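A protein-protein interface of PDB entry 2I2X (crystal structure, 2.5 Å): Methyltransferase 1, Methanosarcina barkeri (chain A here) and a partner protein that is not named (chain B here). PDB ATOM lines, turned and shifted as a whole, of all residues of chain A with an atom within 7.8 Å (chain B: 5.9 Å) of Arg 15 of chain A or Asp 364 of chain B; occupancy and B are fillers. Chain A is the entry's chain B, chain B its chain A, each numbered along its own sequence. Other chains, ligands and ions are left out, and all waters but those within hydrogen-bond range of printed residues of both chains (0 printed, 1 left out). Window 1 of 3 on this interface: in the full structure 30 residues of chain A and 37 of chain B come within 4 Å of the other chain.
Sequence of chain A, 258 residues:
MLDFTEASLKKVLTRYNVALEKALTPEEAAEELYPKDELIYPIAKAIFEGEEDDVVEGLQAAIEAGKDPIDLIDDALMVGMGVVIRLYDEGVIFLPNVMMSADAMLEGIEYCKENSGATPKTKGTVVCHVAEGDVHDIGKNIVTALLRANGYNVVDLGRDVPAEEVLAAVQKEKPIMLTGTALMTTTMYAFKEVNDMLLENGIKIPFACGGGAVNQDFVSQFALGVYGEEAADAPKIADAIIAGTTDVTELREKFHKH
The side-chain carboxylate of Glu 418 of chain B lies within hydrogen-bond range of the backbone NH of Ser 415 of chain B. A ring nitrogen (ND1) of His 240 of chain B lies within hydrogen-bond range of the side-chain carboxylate (OD2) of Asp 364 of chain B (2.5 Å). OD1 of Asp 360 of chain B lies within salt-bridge range of NE of Arg 363 of chain B, at 2.9 Å. The side-chain carboxylate (OD1) of Asp 364 of chain B lies within hydrogen-bond range of the backbone NH (N) of Gln 366 of chain B, at 3.0 Å. The side-chain amide nitrogen of Asn 17 of chain A sits close to the backbone carbonyl oxygen of Arg 15 of chain A, at 3.4 Å.
NH1 of Arg 15 of chain A is in hydrogen-bond range of O of Glu 413 of chain B. O of Arg 363 of chain B sits at hydrogen-bond distance from NE of Arg 15 of chain A. OE2 of Glu 418 of chain B is in salt-bridge range of NH2 of Arg 15 of chain A (2.9 Å). The side-chain carboxylate (OD2) of Asp 364 of chain B is in salt-bridge range of the guanidinium group (NH2) of Arg 15 of chain A, 3.0 Å away.
Printed residues of chain A that touch a printed residue of chain B: Leu 9, Leu 13, Arg 15, Asn 17 and Val 18. Hydrophobic or aromatic side chains of chain A that line the printed part of chain B: Leu 9, Leu 13 and Val 18. Of the 18 printed residues of chain B, 9 touch a printed residue of chain A. Hydrophobic or aromatic side chains of chain B that line the printed part of chain A: Leu 233, Tyr 362 and Pro 365. Along chain B the printed residues that touch a printed residue of chain A span positions 233 to 418.
Arg 15 of chain A touches eight residues of chain B. Asp 364 of chain B touches one residue of chain A. Of the printed residues of chain A, Leu 414 of chain B touches Arg 15. Of the printed residues of chain A, Leu 233 of chain B touches Arg 15 and Asn 17. Of the printed residues of chain B, Asn 17 of chain A touches Leu 233 and Glu 418. Of the printed residues of chain A, Arg 363 of chain B touches Leu 13 (3.6 Å) and Arg 15 (2.8 Å). The nearest printed residue of chain A that does not touch Leu 233 of chain B is Thr 14 of chain A (4.1 Å).
Among the printed residues, merely in contact across the chains: Leu 9 of chain A with Tyr 362 of chain B (3.7 Å), Leu 13 of chain A with Tyr 362 of chain B (3.9 Å), Leu 13 of chain A with Arg 363 of chain B (3.6 Å), Arg 15 of chain A with Leu 233 of chain B (3.9 Å), Arg 15 of chain A with Tyr 362 of chain B (3.5 Å), Arg 15 of chain A with Pro 365 of chain B (3.9 Å), Arg 15 of chain A with Leu 414 of chain B (3.9 Å), Asn 17 of chain A with Leu 233 of chain B (3.1 Å), Asn 17 of chain A with Glu 418 of chain B (3.8 Å), Val 18 of chain A with Glu 413 of chain B (3.6 Å) and Val 18 of chain A with Ser 415 of chain B (3.8 Å).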
ATOM      1  N   LEU A   9      13.614  14.014 -10.740  1.00  0.00           N
ATOM      2  CA  LEU A   9      15.053  14.078 -10.937  1.00  0.00           C
ATOM      3  C   LEU A   9      15.410  13.665 -12.377  1.00  0.00           C
ATOM      4  O   LEU A   9      16.207  14.313 -13.066  1.00  0.00           O
ATOM      5  CB  LEU A   9      15.775  13.163  -9.950  1.00  0.00           C
ATOM      6  CG  LEU A   9      17.241  13.427  -9.594  1.00  0.00           C
ATOM      7  CD1 LEU A   9      17.942  12.165  -9.221  1.00  0.00           C
ATOM      8  CD2 LEU A   9      18.033  14.161 -10.643  1.00  0.00           C
ATOM      9  N   LYS A  10      14.827  12.565 -12.824  1.00  0.00           N
ATOM     10  CA  LYS A  10      15.111  12.049 -14.150  1.00  0.00           C
ATOM     11  C   LYS A  10      14.826  13.103 -15.213  1.00  0.00           C
ATOM     12  O   LYS A  10      15.546  13.159 -16.184  1.00  0.00           O
ATOM     13  CB  LYS A  10      14.310  10.775 -14.402  1.00  0.00           C
ATOM     14  CG  LYS A  10      14.712  10.020 -15.643  1.00  0.00           C
ATOM     15  CD  LYS A  10      13.873   8.748 -15.714  1.00  0.00           C
ATOM     16  CE  LYS A  10      14.610   7.615 -16.387  1.00  0.00           C
ATOM     17  NZ  LYS A  10      14.450   7.729 -17.840  1.00  0.00           N
ATOM     18  N   LEU A  13      17.959  16.537 -14.850  1.00  0.00           N
ATOM     19  CA  LEU A  13      19.321  16.402 -15.317  1.00  0.00           C
ATOM     20  C   LEU A  13      19.577  14.940 -15.738  1.00  0.00           C
ATOM     21  O   LEU A  13      18.731  14.067 -15.516  1.00  0.00           O
ATOM     22  CB  LEU A  13      20.297  16.875 -14.219  1.00  0.00           C
ATOM     23  CG  LEU A  13      20.266  16.116 -12.888  1.00  0.00           C
ATOM     24  CD1 LEU A  13      21.152  14.820 -12.875  1.00  0.00           C
ATOM     25  CD2 LEU A  13      20.646  16.997 -11.706  1.00  0.00           C
ATOM     26  N   THR A  14      20.737  14.677 -16.330  1.00  0.00           N
ATOM     27  CA  THR A  14      21.167  13.328 -16.628  1.00  0.00           C
ATOM     28  C   THR A  14      22.672  13.224 -16.380  1.00  0.00           C
ATOM     29  O   THR A  14      23.439  13.921 -17.032  1.00  0.00           O
ATOM     30  CB  THR A  14      20.906  12.987 -18.122  1.00  0.00           C
ATOM     31  OG1 THR A  14      19.517  12.979 -18.345  1.00  0.00           O
ATOM     32  CG2 THR A  14      21.437  11.590 -18.495  1.00  0.00           C
ATOM     33  N   ARG A  15      23.104  12.346 -15.476  1.00  0.00           N
ATOM     34  CA  ARG A  15      24.539  12.059 -15.353  1.00  0.00           C
ATOM     35  C   ARG A  15      24.883  11.109 -16.474  1.00  0.00           C
ATOM     36  O   ARG A  15      24.870   9.887 -16.321  1.00  0.00           O
ATOM     37  CB  ARG A  15      24.923  11.495 -13.959  1.00  0.00           C
ATOM     38  CG  ARG A  15      24.579  12.464 -12.789  1.00  0.00           C
ATOM     39  CD  ARG A  15      25.414  12.215 -11.534  1.00  0.00           C
ATOM     40  NE  ARG A  15      26.818  12.617 -11.640  1.00  0.00           N
ATOM     41  CZ  ARG A  15      27.839  11.780 -11.523  1.00  0.00           C
ATOM     42  NH1 ARG A  15      27.606  10.491 -11.304  1.00  0.00           N
ATOM     43  NH2 ARG A  15      29.098  12.214 -11.651  1.00  0.00           N
ATOM     44  N   TYR A  16      25.210  11.693 -17.619  1.00  0.00           N
ATOM     45  CA  TYR A  16      25.400  10.955 -18.863  1.00  0.00           C
ATOM     46  C   TYR A  16      26.467   9.873 -18.761  1.00  0.00           C
ATOM     47  O   TYR A  16      26.497   8.948 -19.582  1.00  0.00           O
ATOM     48  CB  TYR A  16      25.727  11.912 -20.005  1.00  0.00           C
ATOM     49  CG  TYR A  16      24.560  12.726 -20.507  1.00  0.00           C
ATOM     50  CD1 TYR A  16      23.665  12.202 -21.450  1.00  0.00           C
ATOM     51  CD2 TYR A  16      24.357  14.034 -20.076  1.00  0.00           C
ATOM     52  CE1 TYR A  16      22.581  12.963 -21.946  1.00  0.00           C
ATOM     53  CE2 TYR A  16      23.278  14.799 -20.560  1.00  0.00           C
ATOM     54  CZ  TYR A  16      22.397  14.256 -21.493  1.00  0.00           C
ATOM     55  OH  TYR A  16      21.335  15.011 -21.973  1.00  0.00           O
ATOM     56  N   ASN A  17      27.351   9.985 -17.774  1.00  0.00           N
ATOM     57  CA  ASN A  17      28.500   9.085 -17.709  1.00  0.00           C
ATOM     58  C   ASN A  17      28.046   7.721 -17.247  1.00  0.00           C
ATOM     59  O   ASN A  17      28.612   6.711 -17.615  1.00  0.00           O
ATOM     60  CB  ASN A  17      29.598   9.623 -16.773  1.00  0.00           C
ATOM     61  CG  ASN A  17      29.055  10.048 -15.421  1.00  0.00           C
ATOM     62  OD1 ASN A  17      29.588   9.677 -14.388  1.00  0.00           O
ATOM     63  ND2 ASN A  17      27.977  10.815 -15.422  1.00  0.00           N
ATOM     64  N   VAL A  18      27.005   7.695 -16.441  1.00  0.00           N
ATOM     65  CA  VAL A  18      26.588   6.455 -15.817  1.00  0.00           C
ATOM     66  C   VAL A  18      26.197   5.342 -16.829  1.00  0.00           C
ATOM     67  O   VAL A  18      26.699   4.223 -16.731  1.00  0.00           O
ATOM     68  CB  VAL A  18      25.504   6.752 -14.783  1.00  0.00           C
ATOM     69  CG1 VAL A  18      24.804   5.466 -14.313  1.00  0.00           C
ATOM     70  CG2 VAL A  18      26.149   7.470 -13.627  1.00  0.00           C
ATOM     71  N   ALA A  19      25.339   5.664 -17.801  1.00  0.00           N
ATOM     72  CA  ALA A  19      24.843   4.666 -18.760  1.00  0.00           C
ATOM     73  C   ALA A  19      25.937   4.208 -19.691  1.00  0.00           C
ATOM     74  O   ALA A  19      25.908   3.074 -20.173  1.00  0.00           O
ATOM     75  CB  ALA A  19      23.638   5.192 -19.564  1.00  0.00           C
ATOM     76  N   LEU A  20      26.907   5.090 -19.924  1.00  0.00           N
ATOM     77  CA  LEU A  20      28.016   4.839 -20.842  1.00  0.00           C
ATOM     78  C   LEU A  20      29.077   3.930 -20.273  1.00  0.00           C
ATOM     79  O   LEU A  20      29.922   3.446 -21.032  1.00  0.00           O
ATOM     80  CB  LEU A  20      28.702   6.142 -21.253  1.00  0.00           C
ATOM     81  CG  LEU A  20      28.040   7.088 -22.239  1.00  0.00           C
ATOM     82  CD1 LEU A  20      29.148   7.919 -22.821  1.00  0.00           C
ATOM     83  CD2 LEU A  20      27.301   6.376 -23.353  1.00  0.00           C
ATOM     84  N   LEU B 233      31.345  15.595 -16.421  1.00  0.00           N
ATOM     85  CA  LEU B 233      30.868  14.243 -16.136  1.00  0.00           C
ATOM     86  C   LEU B 233      31.518  13.119 -16.939  1.00  0.00           C
ATOM     87  O   LEU B 233      31.531  12.002 -16.474  1.00  0.00           O
ATOM     88  CB  LEU B 233      29.365  14.166 -16.373  1.00  0.00           C
ATOM     89  CG  LEU B 233      28.352  14.494 -15.272  1.00  0.00           C
ATOM     90  CD1 LEU B 233      28.910  15.316 -14.084  1.00  0.00           C
ATOM     91  CD2 LEU B 233      27.176  15.184 -15.958  1.00  0.00           C
ATOM     92  N   HIS B 240      35.288  12.012  -9.648  1.00  0.00           N
ATOM     93  CA  HIS B 240      34.622  13.095  -8.995  1.00  0.00           C
ATOM     94  C   HIS B 240      34.488  12.842  -7.507  1.00  0.00           C
ATOM     95  O   HIS B 240      34.517  13.794  -6.698  1.00  0.00           O
ATOM     96  CB  HIS B 240      33.312  13.395  -9.713  1.00  0.00           C
ATOM     97  CG  HIS B 240      33.512  14.051 -11.053  1.00  0.00           C
ATOM     98  ND1 HIS B 240      32.510  14.736 -11.713  1.00  0.00           N
ATOM     99  CD2 HIS B 240      34.608  14.137 -11.846  1.00  0.00           C
ATOM    100  CE1 HIS B 240      32.980  15.208 -12.858  1.00  0.00           C
ATOM    101  NE2 HIS B 240      34.247  14.851 -12.966  1.00  0.00           N
ATOM    102  N   VAL B 298      29.768  22.141 -11.975  1.00  0.00           N
ATOM    103  CA  VAL B 298      28.740  21.139 -11.955  1.00  0.00           C
ATOM    104  C   VAL B 298      27.781  21.460 -10.828  1.00  0.00           C
ATOM    105  O   VAL B 298      26.961  20.607 -10.432  1.00  0.00           O
ATOM    106  CB  VAL B 298      29.401  19.759 -11.896  1.00  0.00           C
ATOM    107  CG1 VAL B 298      29.749  19.324 -10.451  1.00  0.00           C
ATOM    108  CG2 VAL B 298      28.627  18.753 -12.654  1.00  0.00           C
ATOM    109  N   ASP B 360      20.949  21.277  -8.312  1.00  0.00           N
ATOM    110  CA  ASP B 360      22.232  20.665  -8.571  1.00  0.00           C
ATOM    111  C   ASP B 360      22.578  19.551  -7.599  1.00  0.00           C
ATOM    112  O   ASP B 360      23.548  18.850  -7.838  1.00  0.00           O
ATOM    113  CB  ASP B 360      23.329  21.732  -8.535  1.00  0.00           C
ATOM    114  CG  ASP B 360      23.164  22.776  -9.629  1.00  0.00           C
ATOM    115  OD1 ASP B 360      22.594  22.434 -10.671  1.00  0.00           O
ATOM    116  OD2 ASP B 360      23.622  23.931  -9.463  1.00  0.00           O
ATOM    117  N   ARG B 361      21.795  19.377  -6.525  1.00  0.00           N
ATOM    118  CA  ARG B 361      22.085  18.349  -5.533  1.00  0.00           C
ATOM    119  C   ARG B 361      22.469  16.990  -6.157  1.00  0.00           C
ATOM    120  O   ARG B 361      23.340  16.285  -5.597  1.00  0.00           O
ATOM    121  CB  ARG B 361      20.943  18.176  -4.471  1.00  0.00           C
ATOM    122  CG  ARG B 361      21.071  16.846  -3.643  1.00  0.00           C
ATOM    123  CD  ARG B 361      19.985  16.587  -2.560  1.00  0.00           C
ATOM    124  NE  ARG B 361      20.238  17.569  -1.553  1.00  0.00           N
ATOM    125  CZ  ARG B 361      20.529  17.375  -0.279  1.00  0.00           C
ATOM    126  NH1 ARG B 361      20.546  16.172   0.273  1.00  0.00           N
ATOM    127  NH2 ARG B 361      20.763  18.463   0.444  1.00  0.00           N
ATOM    128  N   TYR B 362      21.837  16.623  -7.284  1.00  0.00           N
ATOM    129  CA  TYR B 362      22.050  15.273  -7.847  1.00  0.00           C
ATOM    130  C   TYR B 362      22.954  15.247  -9.083  1.00  0.00           C
ATOM    131  O   TYR B 362      23.238  14.172  -9.655  1.00  0.00           O
ATOM    132  CB  TYR B 362      20.714  14.532  -8.093  1.00  0.00           C
ATOM    133  CG  TYR B 362      19.929  14.302  -6.804  1.00  0.00           C
ATOM    134  CD1 TYR B 362      20.363  13.369  -5.844  1.00  0.00           C
ATOM    135  CD2 TYR B 362      18.778  15.051  -6.521  1.00  0.00           C
ATOM    136  CE1 TYR B 362      19.654  13.179  -4.647  1.00  0.00           C
ATOM    137  CE2 TYR B 362      18.072  14.875  -5.332  1.00  0.00           C
ATOM    138  CZ  TYR B 362      18.500  13.929  -4.406  1.00  0.00           C
ATOM    139  OH  TYR B 362      17.790  13.767  -3.235  1.00  0.00           O
ATOM    140  N   ARG B 363      23.421  16.429  -9.470  1.00  0.00           N
ATOM    141  CA  ARG B 363      24.259  16.538 -10.627  1.00  0.00           C
ATOM    142  C   ARG B 363      25.586  15.789 -10.496  1.00  0.00           C
ATOM    143  O   ARG B 363      26.062  15.258 -11.497  1.00  0.00           O
ATOM    144  CB  ARG B 363      24.519  18.002 -10.966  1.00  0.00           C
ATOM    145  CG  ARG B 363      24.712  18.303 -12.478  1.00  0.00           C
ATOM    146  CD  ARG B 363      24.765  19.825 -12.689  1.00  0.00           C
ATOM    147  NE  ARG B 363      23.410  20.336 -12.577  1.00  0.00           N
ATOM    148  CZ  ARG B 363      22.504  20.291 -13.557  1.00  0.00           C
ATOM    149  NH1 ARG B 363      22.787  19.752 -14.751  1.00  0.00           N
ATOM    150  NH2 ARG B 363      21.296  20.738 -13.319  1.00  0.00           N
ATOM    151  N   ASP B 364      26.175  15.744  -9.289  1.00  0.00           N
ATOM    152  CA  ASP B 364      27.548  15.252  -9.088  1.00  0.00           C
ATOM    153  C   ASP B 364      27.841  15.158  -7.591  1.00  0.00           C
ATOM    154  O   ASP B 364      27.275  15.922  -6.810  1.00  0.00           O
ATOM    155  CB  ASP B 364      28.534  16.238  -9.694  1.00  0.00           C
ATOM    156  CG  ASP B 364      29.896  15.628  -9.972  1.00  0.00           C
ATOM    157  OD1 ASP B 364      30.801  15.840  -9.137  1.00  0.00           O
ATOM    158  OD2 ASP B 364      30.072  14.935 -11.014  1.00  0.00           O
ATOM    159  N   PRO B 365      28.730  14.227  -7.172  1.00  0.00           N
ATOM    160  CA  PRO B 365      29.047  14.229  -5.744  1.00  0.00           C
ATOM    161  C   PRO B 365      29.671  15.533  -5.265  1.00  0.00           C
ATOM    162  O   PRO B 365      29.508  15.897  -4.095  1.00  0.00           O
ATOM    163  CB  PRO B 365      30.017  13.037  -5.591  1.00  0.00           C
ATOM    164  CG  PRO B 365      30.522  12.770  -6.934  1.00  0.00           C
ATOM    165  CD  PRO B 365      29.430  13.125  -7.878  1.00  0.00           C
ATOM    166  N   GLN B 366      30.366  16.236  -6.151  1.00  0.00           N
ATOM    167  CA  GLN B 366      30.946  17.547  -5.795  1.00  0.00           C
ATOM    168  C   GLN B 366      29.863  18.552  -5.401  1.00  0.00           C
ATOM    169  O   GLN B 366      30.097  19.453  -4.596  1.00  0.00           O
ATOM    170  CB  GLN B 366      31.779  18.113  -6.939  1.00  0.00           C
ATOM    171  CG  GLN B 366      33.003  17.279  -7.247  1.00  0.00           C
ATOM    172  CD  GLN B 366      33.820  17.840  -8.393  1.00  0.00           C
ATOM    173  OE1 GLN B 366      34.661  18.724  -8.196  1.00  0.00           O
ATOM    174  NE2 GLN B 366      33.612  17.300  -9.590  1.00  0.00           N
ATOM    175  N   ALA B 367      28.665  18.379  -5.950  1.00  0.00           N
ATOM    176  CA  ALA B 367      27.593  19.301  -5.676  1.00  0.00           C
ATOM    177  C   ALA B 367      26.822  18.813  -4.449  1.00  0.00           C
ATOM    178  O   ALA B 367      26.536  19.604  -3.514  1.00  0.00           O
ATOM    179  CB  ALA B 367      26.707  19.423  -6.882  1.00  0.00           C
ATOM    180  N   TYR B 368      26.513  17.513  -4.444  1.00  0.00           N
ATOM    181  CA  TYR B 368      25.821  16.890  -3.332  1.00  0.00           C
ATOM    182  C   TYR B 368      26.354  17.303  -1.948  1.00  0.00           C
ATOM    183  O   TYR B 368      25.577  17.677  -1.063  1.00  0.00           O
ATOM    184  CB  TYR B 368      25.865  15.357  -3.469  1.00  0.00           C
ATOM    185  CG  TYR B 368      24.905  14.677  -2.524  1.00  0.00           C
ATOM    186  CD1 TYR B 368      23.575  14.456  -2.904  1.00  0.00           C
ATOM    187  CD2 TYR B 368      25.307  14.291  -1.242  1.00  0.00           C
ATOM    188  CE1 TYR B 368      22.663  13.884  -2.046  1.00  0.00           C
ATOM    189  CE2 TYR B 368      24.382  13.685  -0.360  1.00  0.00           C
ATOM    190  CZ  TYR B 368      23.066  13.498  -0.779  1.00  0.00           C
ATOM    191  OH  TYR B 368      22.151  12.913   0.043  1.00  0.00           O
ATOM    192  N   MET B 369      27.670  17.216  -1.759  1.00  0.00           N
ATOM    193  CA  MET B 369      28.307  17.565  -0.491  1.00  0.00           C
ATOM    194  C   MET B 369      28.181  19.053  -0.190  1.00  0.00           C
ATOM    195  O   MET B 369      28.093  19.458   0.962  1.00  0.00           O
ATOM    196  CB  MET B 369      29.784  17.160  -0.519  1.00  0.00           C
ATOM    197  CG  MET B 369      30.540  17.312   0.825  1.00  0.00           C
ATOM    198  SD  MET B 369      31.281  18.960   1.089  1.00  0.00           S
ATOM    199  CE  MET B 369      32.808  18.782   0.196  1.00  0.00           C
ATOM    200  N   LEU B 412      21.316   9.873  -5.556  1.00  0.00           N
ATOM    201  CA  LEU B 412      22.594  10.220  -6.192  1.00  0.00           C
ATOM    202  C   LEU B 412      23.087   9.006  -6.980  1.00  0.00           C
ATOM    203  O   LEU B 412      23.321   7.941  -6.411  1.00  0.00           O
ATOM    204  CB  LEU B 412      23.649  10.638  -5.144  1.00  0.00           C
ATOM    205  CG  LEU B 412      25.026  11.105  -5.655  1.00  0.00           C
ATOM    206  CD1 LEU B 412      24.926  12.329  -6.600  1.00  0.00           C
ATOM    207  CD2 LEU B 412      26.022  11.374  -4.531  1.00  0.00           C
ATOM    208  N   GLU B 413      23.233   9.180  -8.287  1.00  0.00           N
ATOM    209  CA  GLU B 413      23.539   8.101  -9.197  1.00  0.00           C
ATOM    210  C   GLU B 413      25.035   8.153  -9.554  1.00  0.00           C
ATOM    211  O   GLU B 413      25.468   8.937 -10.415  1.00  0.00           O
ATOM    212  CB  GLU B 413      22.651   8.274 -10.427  1.00  0.00           C
ATOM    213  CG  GLU B 413      22.537   7.096 -11.367  1.00  0.00           C
ATOM    214  CD  GLU B 413      21.910   7.476 -12.707  1.00  0.00           C
ATOM    215  OE1 GLU B 413      21.948   8.664 -13.124  1.00  0.00           O
ATOM    216  OE2 GLU B 413      21.366   6.578 -13.374  1.00  0.00           O
ATOM    217  N   LEU B 414      25.832   7.322  -8.877  1.00  0.00           N
ATOM    218  CA  LEU B 414      27.271   7.279  -9.113  1.00  0.00           C
ATOM    219  C   LEU B 414      27.578   6.156 -10.067  1.00  0.00           C
ATOM    220  O   LEU B 414      26.920   5.120 -10.012  1.00  0.00           O
ATOM    221  CB  LEU B 414      28.013   7.019  -7.807  1.00  0.00           C
ATOM    222  CG  LEU B 414      27.863   7.969  -6.627  1.00  0.00           C
ATOM    223  CD1 LEU B 414      28.909   7.584  -5.594  1.00  0.00           C
ATOM    224  CD2 LEU B 414      28.032   9.446  -7.092  1.00  0.00           C
ATOM    225  N   SER B 415      28.587   6.338 -10.916  1.00  0.00           N
ATOM    226  CA  SER B 415      29.100   5.227 -11.699  1.00  0.00           C
ATOM    227  C   SER B 415      29.856   4.219 -10.796  1.00  0.00           C
ATOM    228  O   SER B 415      30.245   4.557  -9.662  1.00  0.00           O
ATOM    229  CB  SER B 415      30.028   5.721 -12.799  1.00  0.00           C
ATOM    230  OG  SER B 415      31.233   6.201 -12.234  1.00  0.00           O
ATOM    231  N   GLU B 418      33.216   5.611  -9.887  1.00  0.00           N
ATOM    232  CA  GLU B 418      33.143   6.623  -8.843  1.00  0.00           C
ATOM    233  C   GLU B 418      32.990   5.989  -7.482  1.00  0.00           C
ATOM    234  O   GLU B 418      33.527   6.499  -6.506  1.00  0.00           O
ATOM    235  CB  GLU B 418      31.978   7.584  -9.091  1.00  0.00           C
ATOM    236  CG  GLU B 418      32.348   8.653 -10.059  1.00  0.00           C
ATOM    237  CD  GLU B 418      31.179   9.385 -10.687  1.00  0.00           C
ATOM    238  OE1 GLU B 418      30.040   8.858 -10.706  1.00  0.00           O
ATOM    239  OE2 GLU B 418      31.424  10.506 -11.175  1.00  0.00           O
